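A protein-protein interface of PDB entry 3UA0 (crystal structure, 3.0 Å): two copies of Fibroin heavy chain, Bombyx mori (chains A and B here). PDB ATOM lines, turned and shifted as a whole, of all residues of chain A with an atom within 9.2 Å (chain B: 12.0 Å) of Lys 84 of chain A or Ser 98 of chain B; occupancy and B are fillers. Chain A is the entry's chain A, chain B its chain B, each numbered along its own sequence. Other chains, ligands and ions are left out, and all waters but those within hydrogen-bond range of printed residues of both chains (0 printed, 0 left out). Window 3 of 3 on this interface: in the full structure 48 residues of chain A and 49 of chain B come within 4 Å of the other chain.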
ATOM      1  N   ASN A  76     -32.279   5.405 -19.280  1.00  0.00           N
ATOM      2  CA  ASN A  76     -31.969   4.268 -20.139  1.00  0.00           C
ATOM      3  C   ASN A  76     -31.930   4.571 -21.641  1.00  0.00           C
ATOM      4  O   ASN A  76     -30.874   4.469 -22.274  1.00  0.00           O
ATOM      5  CB  ASN A  76     -32.915   3.108 -19.825  1.00  0.00           C
ATOM      6  CG  ASN A  76     -32.202   1.772 -19.827  1.00  0.00           C
ATOM      7  OD1 ASN A  76     -31.209   1.592 -20.529  1.00  0.00           O
ATOM      8  ND2 ASN A  76     -32.707   0.831 -19.035  1.00  0.00           N
ATOM      9  N   ILE A  81     -21.445   7.637 -25.409  1.00  0.00           N
ATOM     10  CA  ILE A  81     -21.801   6.795 -24.274  1.00  0.00           C
ATOM     11  C   ILE A  81     -20.782   5.673 -24.048  1.00  0.00           C
ATOM     12  O   ILE A  81     -21.144   4.496 -24.012  1.00  0.00           O
ATOM     13  CB  ILE A  81     -23.242   6.202 -24.408  1.00  0.00           C
ATOM     14  CG1 ILE A  81     -23.360   5.279 -25.629  1.00  0.00           C
ATOM     15  CG2 ILE A  81     -24.278   7.314 -24.486  1.00  0.00           C
ATOM     16  CD1 ILE A  81     -23.531   6.007 -26.955  1.00  0.00           C
ATOM     17  N   LEU A  82     -19.510   6.038 -23.900  1.00  0.00           N
ATOM     18  CA  LEU A  82     -18.493   5.046 -23.556  1.00  0.00           C
ATOM     19  C   LEU A  82     -19.000   4.249 -22.360  1.00  0.00           C
ATOM     20  O   LEU A  82     -19.498   4.818 -21.384  1.00  0.00           O
ATOM     21  CB  LEU A  82     -17.124   5.693 -23.261  1.00  0.00           C
ATOM     22  CG  LEU A  82     -16.093   5.853 -24.398  1.00  0.00           C
ATOM     23  CD1 LEU A  82     -14.743   6.385 -23.889  1.00  0.00           C
ATOM     24  CD2 LEU A  82     -15.894   4.542 -25.165  1.00  0.00           C
ATOM     25  N   GLY A  83     -18.912   2.929 -22.461  1.00  0.00           N
ATOM     26  CA  GLY A  83     -19.354   2.054 -21.393  1.00  0.00           C
ATOM     27  C   GLY A  83     -18.194   1.255 -20.834  1.00  0.00           C
ATOM     28  O   GLY A  83     -17.297   1.806 -20.192  1.00  0.00           O
ATOM     29  N   LYS A  84     -18.217  -0.050 -21.082  1.00  0.00           N
ATOM     30  CA  LYS A  84     -17.143  -0.948 -20.666  1.00  0.00           C
ATOM     31  C   LYS A  84     -16.880  -0.874 -19.159  1.00  0.00           C
ATOM     32  O   LYS A  84     -17.543  -1.539 -18.360  1.00  0.00           O
ATOM     33  CB  LYS A  84     -15.844  -0.642 -21.436  1.00  0.00           C
ATOM     34  CG  LYS A  84     -16.012  -0.327 -22.925  1.00  0.00           C
ATOM     35  CD  LYS A  84     -14.701   0.165 -23.511  1.00  0.00           C
ATOM     36  CE  LYS A  84     -14.927   1.245 -24.547  1.00  0.00           C
ATOM     37  NZ  LYS A  84     -13.739   2.139 -24.616  1.00  0.00           N
ATOM     38  N   ASN A  85     -15.900  -0.052 -18.791  1.00  0.00           N
ATOM     39  CA  ASN A  85     -15.407   0.049 -17.419  1.00  0.00           C
ATOM     40  C   ASN A  85     -15.657   1.430 -16.823  1.00  0.00           C
ATOM     41  O   ASN A  85     -14.918   1.877 -15.942  1.00  0.00           O
ATOM     42  CB  ASN A  85     -13.902  -0.261 -17.389  1.00  0.00           C
ATOM     43  CG  ASN A  85     -13.137   0.358 -18.574  1.00  0.00           C
ATOM     44  OD1 ASN A  85     -13.558   1.365 -19.151  1.00  0.00           O
ATOM     45  ND2 ASN A  85     -12.006  -0.251 -18.932  1.00  0.00           N
ATOM     46  N   GLU A  86     -16.704   2.096 -17.304  1.00  0.00           N
ATOM     47  CA  GLU A  86     -16.907   3.513 -17.017  1.00  0.00           C
ATOM     48  C   GLU A  86     -18.188   3.821 -16.231  1.00  0.00           C
ATOM     49  O   GLU A  86     -19.123   3.018 -16.192  1.00  0.00           O
ATOM     50  CB  GLU A  86     -16.840   4.317 -18.322  1.00  0.00           C
ATOM     51  CG  GLU A  86     -15.425   4.388 -18.914  1.00  0.00           C
ATOM     52  CD  GLU A  86     -15.397   4.559 -20.426  1.00  0.00           C
ATOM     53  OE1 GLU A  86     -16.269   3.988 -21.114  1.00  0.00           O
ATOM     54  OE2 GLU A  86     -14.486   5.253 -20.927  1.00  0.00           O
ATOM     55  N   LYS A  87     -18.203   4.988 -15.591  1.00  0.00           N
ATOM     56  CA  LYS A  87     -19.357   5.462 -14.836  1.00  0.00           C
ATOM     57  C   LYS A  87     -19.362   6.996 -14.794  1.00  0.00           C
ATOM     58  O   LYS A  87     -18.358   7.616 -14.450  1.00  0.00           O
ATOM     59  CB  LYS A  87     -19.354   4.873 -13.417  1.00  0.00           C
ATOM     60  CG  LYS A  87     -20.583   5.243 -12.574  1.00  0.00           C
ATOM     61  CD  LYS A  87     -20.547   4.629 -11.173  1.00  0.00           C
ATOM     62  CE  LYS A  87     -20.868   3.134 -11.194  1.00  0.00           C
ATOM     63  NZ  LYS A  87     -20.751   2.524  -9.831  1.00  0.00           N
ATOM     64  N   MET A  88     -20.488   7.606 -15.158  1.00  0.00           N
ATOM     65  CA  MET A  88     -20.617   9.060 -15.099  1.00  0.00           C
ATOM     66  C   MET A  88     -21.275   9.572 -13.828  1.00  0.00           C
ATOM     67  O   MET A  88     -22.276   9.046 -13.372  1.00  0.00           O
ATOM     68  CB  MET A  88     -21.347   9.621 -16.322  1.00  0.00           C
ATOM     69  CG  MET A  88     -20.431  10.384 -17.291  1.00  0.00           C
ATOM     70  SD  MET A  88     -19.311  11.815 -16.494  1.00  0.00           S
ATOM     71  CE  MET A  88     -18.628  12.618 -18.141  1.00  0.00           C
ATOM     72  N   LEU A 110     -15.709  11.020 -14.628  1.00  0.00           N
ATOM     73  CA  LEU A 110     -15.632   9.765 -15.359  1.00  0.00           C
ATOM     74  C   LEU A 110     -14.700   8.807 -14.641  1.00  0.00           C
ATOM     75  O   LEU A 110     -13.591   9.174 -14.270  1.00  0.00           O
ATOM     76  CB  LEU A 110     -15.150   9.984 -16.786  1.00  0.00           C
ATOM     77  CG  LEU A 110     -15.056   8.664 -17.555  1.00  0.00           C
ATOM     78  CD1 LEU A 110     -16.365   7.897 -17.464  1.00  0.00           C
ATOM     79  CD2 LEU A 110     -14.677   8.889 -19.004  1.00  0.00           C
ATOM     80  N   MET A 111     -15.167   7.581 -14.436  1.00  0.00           N
ATOM     81  CA  MET A 111     -14.387   6.594 -13.723  1.00  0.00           C
ATOM     82  C   MET A 111     -14.090   5.418 -14.617  1.00  0.00           C
ATOM     83  O   MET A 111     -14.954   4.574 -14.841  1.00  0.00           O
ATOM     84  CB  MET A 111     -15.141   6.077 -12.512  1.00  0.00           C
ATOM     85  CG  MET A 111     -16.100   7.059 -11.885  1.00  0.00           C
ATOM     86  SD  MET A 111     -16.742   6.268 -10.227  1.00  0.00           S
ATOM     87  CE  MET A 111     -16.473   4.364 -10.675  1.00  0.00           C
ATOM     88  N   LYS A 112     -12.866   5.376 -15.132  1.00  0.00           N
ATOM     89  CA  LYS A 112     -12.355   4.183 -15.781  1.00  0.00           C
ATOM     90  C   LYS A 112     -11.519   3.469 -14.727  1.00  0.00           C
ATOM     91  O   LYS A 112     -10.576   4.035 -14.168  1.00  0.00           O
ATOM     92  CB  LYS A 112     -11.533   4.527 -17.034  1.00  0.00           C
ATOM     93  CG  LYS A 112     -11.519   3.435 -18.117  1.00  0.00           C
ATOM     94  CD  LYS A 112     -10.884   3.925 -19.421  1.00  0.00           C
ATOM     95  CE  LYS A 112     -10.915   2.857 -20.523  1.00  0.00           C
ATOM     96  NZ  LYS A 112     -12.219   2.771 -21.263  1.00  0.00           N
ATOM     97  N   THR A 113     -11.910   2.238 -14.425  1.00  0.00           N
ATOM     98  CA  THR A 113     -11.177   1.402 -13.490  1.00  0.00           C
ATOM     99  C   THR A 113      -9.996   0.744 -14.201  1.00  0.00           C
ATOM    100  O   THR A 113     -10.152   0.102 -15.244  1.00  0.00           O
ATOM    101  CB  THR A 113     -12.096   0.338 -12.877  1.00  0.00           C
ATOM    102  OG1 THR A 113     -12.964  -0.174 -13.893  1.00  0.00           O
ATOM    103  CG2 THR A 113     -12.958   0.947 -11.776  1.00  0.00           C
ATOM    104  N   ALA B  61      -7.857   0.224  -8.366  1.00  0.00           N
ATOM    105  CA  ALA B  61      -7.467   1.529  -8.904  1.00  0.00           C
ATOM    106  C   ALA B  61      -8.442   2.081  -9.949  1.00  0.00           C
ATOM    107  O   ALA B  61      -8.793   1.411 -10.917  1.00  0.00           O
ATOM    108  CB  ALA B  61      -6.043   1.479  -9.471  1.00  0.00           C
ATOM    109  N   VAL B  62      -8.862   3.324  -9.747  1.00  0.00           N
ATOM    110  CA  VAL B  62      -9.757   3.982 -10.683  1.00  0.00           C
ATOM    111  C   VAL B  62      -9.171   5.309 -11.147  1.00  0.00           C
ATOM    112  O   VAL B  62      -8.762   6.143 -10.333  1.00  0.00           O
ATOM    113  CB  VAL B  62     -11.154   4.249 -10.056  1.00  0.00           C
ATOM    114  CG1 VAL B  62     -12.121   4.781 -11.105  1.00  0.00           C
ATOM    115  CG2 VAL B  62     -11.703   2.985  -9.402  1.00  0.00           C
ATOM    116  N   ILE B  63      -9.125   5.490 -12.462  1.00  0.00           N
ATOM    117  CA  ILE B  63      -8.851   6.796 -13.030  1.00  0.00           C
ATOM    118  C   ILE B  63     -10.124   7.604 -12.899  1.00  0.00           C
ATOM    119  O   ILE B  63     -11.216   7.047 -12.837  1.00  0.00           O
ATOM    120  CB  ILE B  63      -8.510   6.722 -14.532  1.00  0.00           C
ATOM    121  CG1 ILE B  63      -7.564   7.864 -14.939  1.00  0.00           C
ATOM    122  CG2 ILE B  63      -9.794   6.750 -15.366  1.00  0.00           C
ATOM    123  CD1 ILE B  63      -7.483   8.092 -16.425  1.00  0.00           C
ATOM    124  N   GLU B  65     -11.779  11.479 -14.412  1.00  0.00           N
ATOM    125  CA  GLU B  65     -11.574  12.656 -15.246  1.00  0.00           C
ATOM    126  C   GLU B  65     -12.574  13.778 -14.926  1.00  0.00           C
ATOM    127  O   GLU B  65     -13.728  13.744 -15.353  1.00  0.00           O
ATOM    128  CB  GLU B  65     -11.583  12.253 -16.726  1.00  0.00           C
ATOM    129  CG  GLU B  65     -10.851  10.915 -16.974  1.00  0.00           C
ATOM    130  CD  GLU B  65     -10.157  10.829 -18.336  1.00  0.00           C
ATOM    131  OE1 GLU B  65     -10.464  11.659 -19.218  1.00  0.00           O
ATOM    132  OE2 GLU B  65      -9.300   9.932 -18.527  1.00  0.00           O
ATOM    133  N   ILE B  94     -26.360  12.996 -10.774  1.00  0.00           N
ATOM    134  CA  ILE B  94     -26.735  11.963 -11.730  1.00  0.00           C
ATOM    135  C   ILE B  94     -25.621  10.947 -11.932  1.00  0.00           C
ATOM    136  O   ILE B  94     -24.566  11.261 -12.475  1.00  0.00           O
ATOM    137  CB  ILE B  94     -27.097  12.547 -13.106  1.00  0.00           C
ATOM    138  CG1 ILE B  94     -28.233  13.563 -12.995  1.00  0.00           C
ATOM    139  CG2 ILE B  94     -27.490  11.436 -14.054  1.00  0.00           C
ATOM    140  CD1 ILE B  94     -27.829  14.908 -12.434  1.00  0.00           C
ATOM    141  N   THR B  95     -25.886   9.726 -11.485  1.00  0.00           N
ATOM    142  CA  THR B  95     -25.006   8.600 -11.706  1.00  0.00           C
ATOM    143  C   THR B  95     -25.531   7.812 -12.895  1.00  0.00           C
ATOM    144  O   THR B  95     -26.669   7.367 -12.895  1.00  0.00           O
ATOM    145  CB  THR B  95     -24.977   7.676 -10.477  1.00  0.00           C
ATOM    146  OG1 THR B  95     -24.820   8.457  -9.285  1.00  0.00           O
ATOM    147  CG2 THR B  95     -23.839   6.681 -10.587  1.00  0.00           C
ATOM    148  N   THR B  96     -24.699   7.663 -13.915  1.00  0.00           N
ATOM    149  CA  THR B  96     -25.043   6.877 -15.090  1.00  0.00           C
ATOM    150  C   THR B  96     -24.023   5.752 -15.212  1.00  0.00           C
ATOM    151  O   THR B  96     -22.917   5.856 -14.693  1.00  0.00           O
ATOM    152  CB  THR B  96     -24.985   7.729 -16.368  1.00  0.00           C
ATOM    153  OG1 THR B  96     -25.421   9.068 -16.089  1.00  0.00           O
ATOM    154  CG2 THR B  96     -25.849   7.116 -17.455  1.00  0.00           C
ATOM    155  N   ASP B  97     -24.383   4.675 -15.898  1.00  0.00           N
ATOM    156  CA  ASP B  97     -23.468   3.544 -16.011  1.00  0.00           C
ATOM    157  C   ASP B  97     -23.417   2.945 -17.418  1.00  0.00           C
ATOM    158  O   ASP B  97     -24.143   3.379 -18.313  1.00  0.00           O
ATOM    159  CB  ASP B  97     -23.802   2.467 -14.972  1.00  0.00           C
ATOM    160  CG  ASP B  97     -25.013   1.631 -15.354  1.00  0.00           C
ATOM    161  OD1 ASP B  97     -25.630   1.902 -16.400  1.00  0.00           O
ATOM    162  OD2 ASP B  97     -25.351   0.694 -14.603  1.00  0.00           O
ATOM    163  N   SER B  98     -22.555   1.942 -17.589  1.00  0.00           N
ATOM    164  CA  SER B  98     -22.315   1.295 -18.884  1.00  0.00           C
ATOM    165  C   SER B  98     -23.535   0.542 -19.427  1.00  0.00           C
ATOM    166  O   SER B  98     -23.454  -0.137 -20.455  1.00  0.00           O
ATOM    167  CB  SER B  98     -21.107   0.357 -18.789  1.00  0.00           C
ATOM    168  OG  SER B  98     -20.987  -0.190 -17.485  1.00  0.00           O
ATOM    169  N   ASP B  99     -24.659   0.672 -18.726  1.00  0.00           N
ATOM    170  CA  ASP B  99     -25.927   0.085 -19.156  1.00  0.00           C
ATOM    171  C   ASP B  99     -27.004   1.161 -19.348  1.00  0.00           C
ATOM    172  O   ASP B  99     -28.192   0.889 -19.188  1.00  0.00           O
ATOM    173  CB  ASP B  99     -26.414  -0.953 -18.135  1.00  0.00           C
ATOM    174  CG  ASP B  99     -25.538  -2.201 -18.091  1.00  0.00           C
ATOM    175  OD1 ASP B  99     -24.588  -2.309 -18.906  1.00  0.00           O
ATOM    176  OD2 ASP B  99     -25.810  -3.077 -17.237  1.00  0.00           O
ATOM    177  N   GLY B 100     -26.585   2.381 -19.678  1.00  0.00           N
ATOM    178  CA  GLY B 100     -27.511   3.485 -19.886  1.00  0.00           C
ATOM    179  C   GLY B 100     -28.316   3.883 -18.657  1.00  0.00           C
ATOM    180  O   GLY B 100     -29.015   4.898 -18.675  1.00  0.00           O
ATOM    181  N   ASN B 101     -28.207   3.088 -17.592  1.00  0.00           N
ATOM    182  CA  ASN B 101     -28.982   3.277 -16.362  1.00  0.00           C
ATOM    183  C   ASN B 101     -28.624   4.528 -15.559  1.00  0.00           C
ATOM    184  O   ASN B 101     -27.524   4.628 -15.019  1.00  0.00           O
ATOM    185  CB  ASN B 101     -28.832   2.051 -15.454  1.00  0.00           C
ATOM    186  CG  ASN B 101     -29.773   0.920 -15.829  1.00  0.00           C
ATOM    187  OD1 ASN B 101     -29.884  -0.074 -15.105  1.00  0.00           O
ATOM    188  ND2 ASN B 101     -30.461   1.068 -16.958  1.00  0.00           N
ATOM    189  N   GLU B 102     -29.566   5.463 -15.462  1.00  0.00           N
ATOM    190  CA  GLU B 102     -29.348   6.697 -14.711  1.00  0.00           C
ATOM    191  C   GLU B 102     -30.081   6.719 -13.381  1.00  0.00           C
ATOM    192  O   GLU B 102     -31.261   6.376 -13.310  1.00  0.00           O
ATOM    193  CB  GLU B 102     -29.797   7.904 -15.519  1.00  0.00           C
ATOM    194  CG  GLU B 102     -28.884   8.249 -16.644  1.00  0.00           C
ATOM    195  CD  GLU B 102     -28.820   9.729 -16.859  1.00  0.00           C
ATOM    196  OE1 GLU B 102     -29.473  10.441 -16.067  1.00  0.00           O
ATOM    197  OE2 GLU B 102     -28.123  10.176 -17.801  1.00  0.00           O
ATOM    198  N   SER B 103     -29.381   7.129 -12.328  1.00  0.00           N
ATOM    199  CA  SER B 103     -30.051   7.418 -11.074  1.00  0.00           C
ATOM    200  C   SER B 103     -29.722   8.836 -10.624  1.00  0.00           C
ATOM    201  O   SER B 103     -28.558   9.201 -10.448  1.00  0.00           O
ATOM    202  CB  SER B 103     -29.742   6.374  -9.994  1.00  0.00           C
ATOM    203  OG  SER B 103     -28.841   6.868  -9.024  1.00  0.00           O
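No position is printed for both chains.
Of the 19 pairs that touch across the chains among the printed residues, none has its exchanged pair printed and touching as well.
The side-chain amide oxygen (OD1) of Asn 76 of chain A sits close to the backbone carbonyl oxygen (O) of Asp 99 of chain B.
N of Asn 76 of chain A lies close to O of Gly 100 of chain B (3.4 Å).
ND2 of Asn 76 of chain A lies close to ND2 of Asn 101 of chain B, 3.1 Å away.
The backbone carbonyl oxygen of Met 88 of chain A sits at hydrogen-bond distance from the backbone NH of Thr 96 of chain B, at 2.8 Å.
The backbone carbonyl oxygen (O) of Leu 110 of chain A lies within hydrogen-bond range of the backbone NH (N) of Glu 65 of chain B (2.9 Å).
The backbone carbonyl oxygen (O) of Lys 112 of chain A sits at hydrogen-bond distance from the backbone NH (N) of Ile 63 of chain B (2.7 Å).
O of Ile 94 of chain B sits close to O of Met 88 of chain A.
The backbone carbonyl oxygen (O) of Leu 110 of chain A sits close to the backbone carbonyl oxygen (O) of Ile 63 of chain B.
Printed residues of chain B within 4 Å of Asn 76 of chain A: Asp 99, Gly 100 and Asn 101.
No residue of chain B comes within 4 Å of Leu 82 of chain A.
Of chain B, only Ser 98 comes within 4 Å of Gly 83 of chain A.
Lys 84 of chain A touches one residue of chain B.
No residue of chain B comes within 4 Å of Asn 85 of chain A.
No residue of chain A comes within 4 Å of Asp 97 of chain B.
Of chain A, only Gly 83 (3.6 Å), Lys 84 (3.7 Å) and Glu 86 (3.9 Å) come within 4 Å of Ser 98 of chain B.
Asp 99 of chain B touches just one residue of chain A: Asn 76 (3.4 Å).
Of the printed residues of chain A, Gly 100 of chain B touches Asn 76 (3.4 Å).
Glu 102 of chain B touches none of the printed residues of chain A.
Ser 103 of chain B touches none of the printed residues of chain A.
The nearest residue of chain A that does not touch Ser 98 of chain B is Leu 82 of chain A (5.2 Å).
N of Gly 83 of chain A sits at hydrogen-bond distance from OE1 of Glu 86 of chain A, at 3.1 Å.
O of Asn 85 of chain A lies within hydrogen-bond range of N of Thr 113 of chain A.
The side-chain carboxylate (OE2) of Glu 86 of chain A lies within salt-bridge range of the side-chain amino group (NZ) of Lys 112 of chain A.
The side-chain hydroxyl (OG1) of Thr 96 of chain B is in hydrogen-bond range of the side-chain carboxylate (OE2) of Glu 102 of chain B, at 3.4 Å.
OD1 of Asp 97 of chain B sits at hydrogen-bond distance from N of Gly 100 of chain B, 3.4 Å away.
N of Asn 101 of chain B sits at hydrogen-bond distance from OD1 of Asp 97 of chain B, at 3.1 Å.
Of the 14 printed residues of chain B, 11 touch a printed residue of chain A.
Of the 13 printed residues of chain A, 10 touch a printed residue of chain B.
Hydrophobic or aromatic side chains of chain A within 4 Å of the printed part of chain B: Met 111.
Along chain A the printed residues that touch a printed residue of chain B span positions 76 to 113.
Among the printed residues, no Asp or Glu carboxylate lies within 4 Å of a Lys or Arg side-chain nitrogen of the other chain.
Among the printed residues, pairs that only touch across the chains: Gly 83 of chain A with Ser 98 of chain B (3.6 Å), Lys 84 of chain A with Ser 98 of chain B (3.7 Å), Glu 86 of chain A with Ser 98 of chain B (3.9 Å), Lys 87 of chain A with Thr 95 of chain B (3.9 Å), Lys 87 of chain A with Thr 96 of chain B (3.2 Å), Met 88 of chain A with Thr 95 of chain B (3.2 Å), Met 111 of chain A with Val 62 of chain B (3.6 Å), Met 111 of chain A with Ile 63 of chain B (3.3 Å), Lys 112 of chain A with Val 62 of chain B (3.5 Å), Thr 113 of chain A with Ala 61 of chain B (3.5 Å) and Thr 113 of chain A with Val 62 of chain B (3.4 Å).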
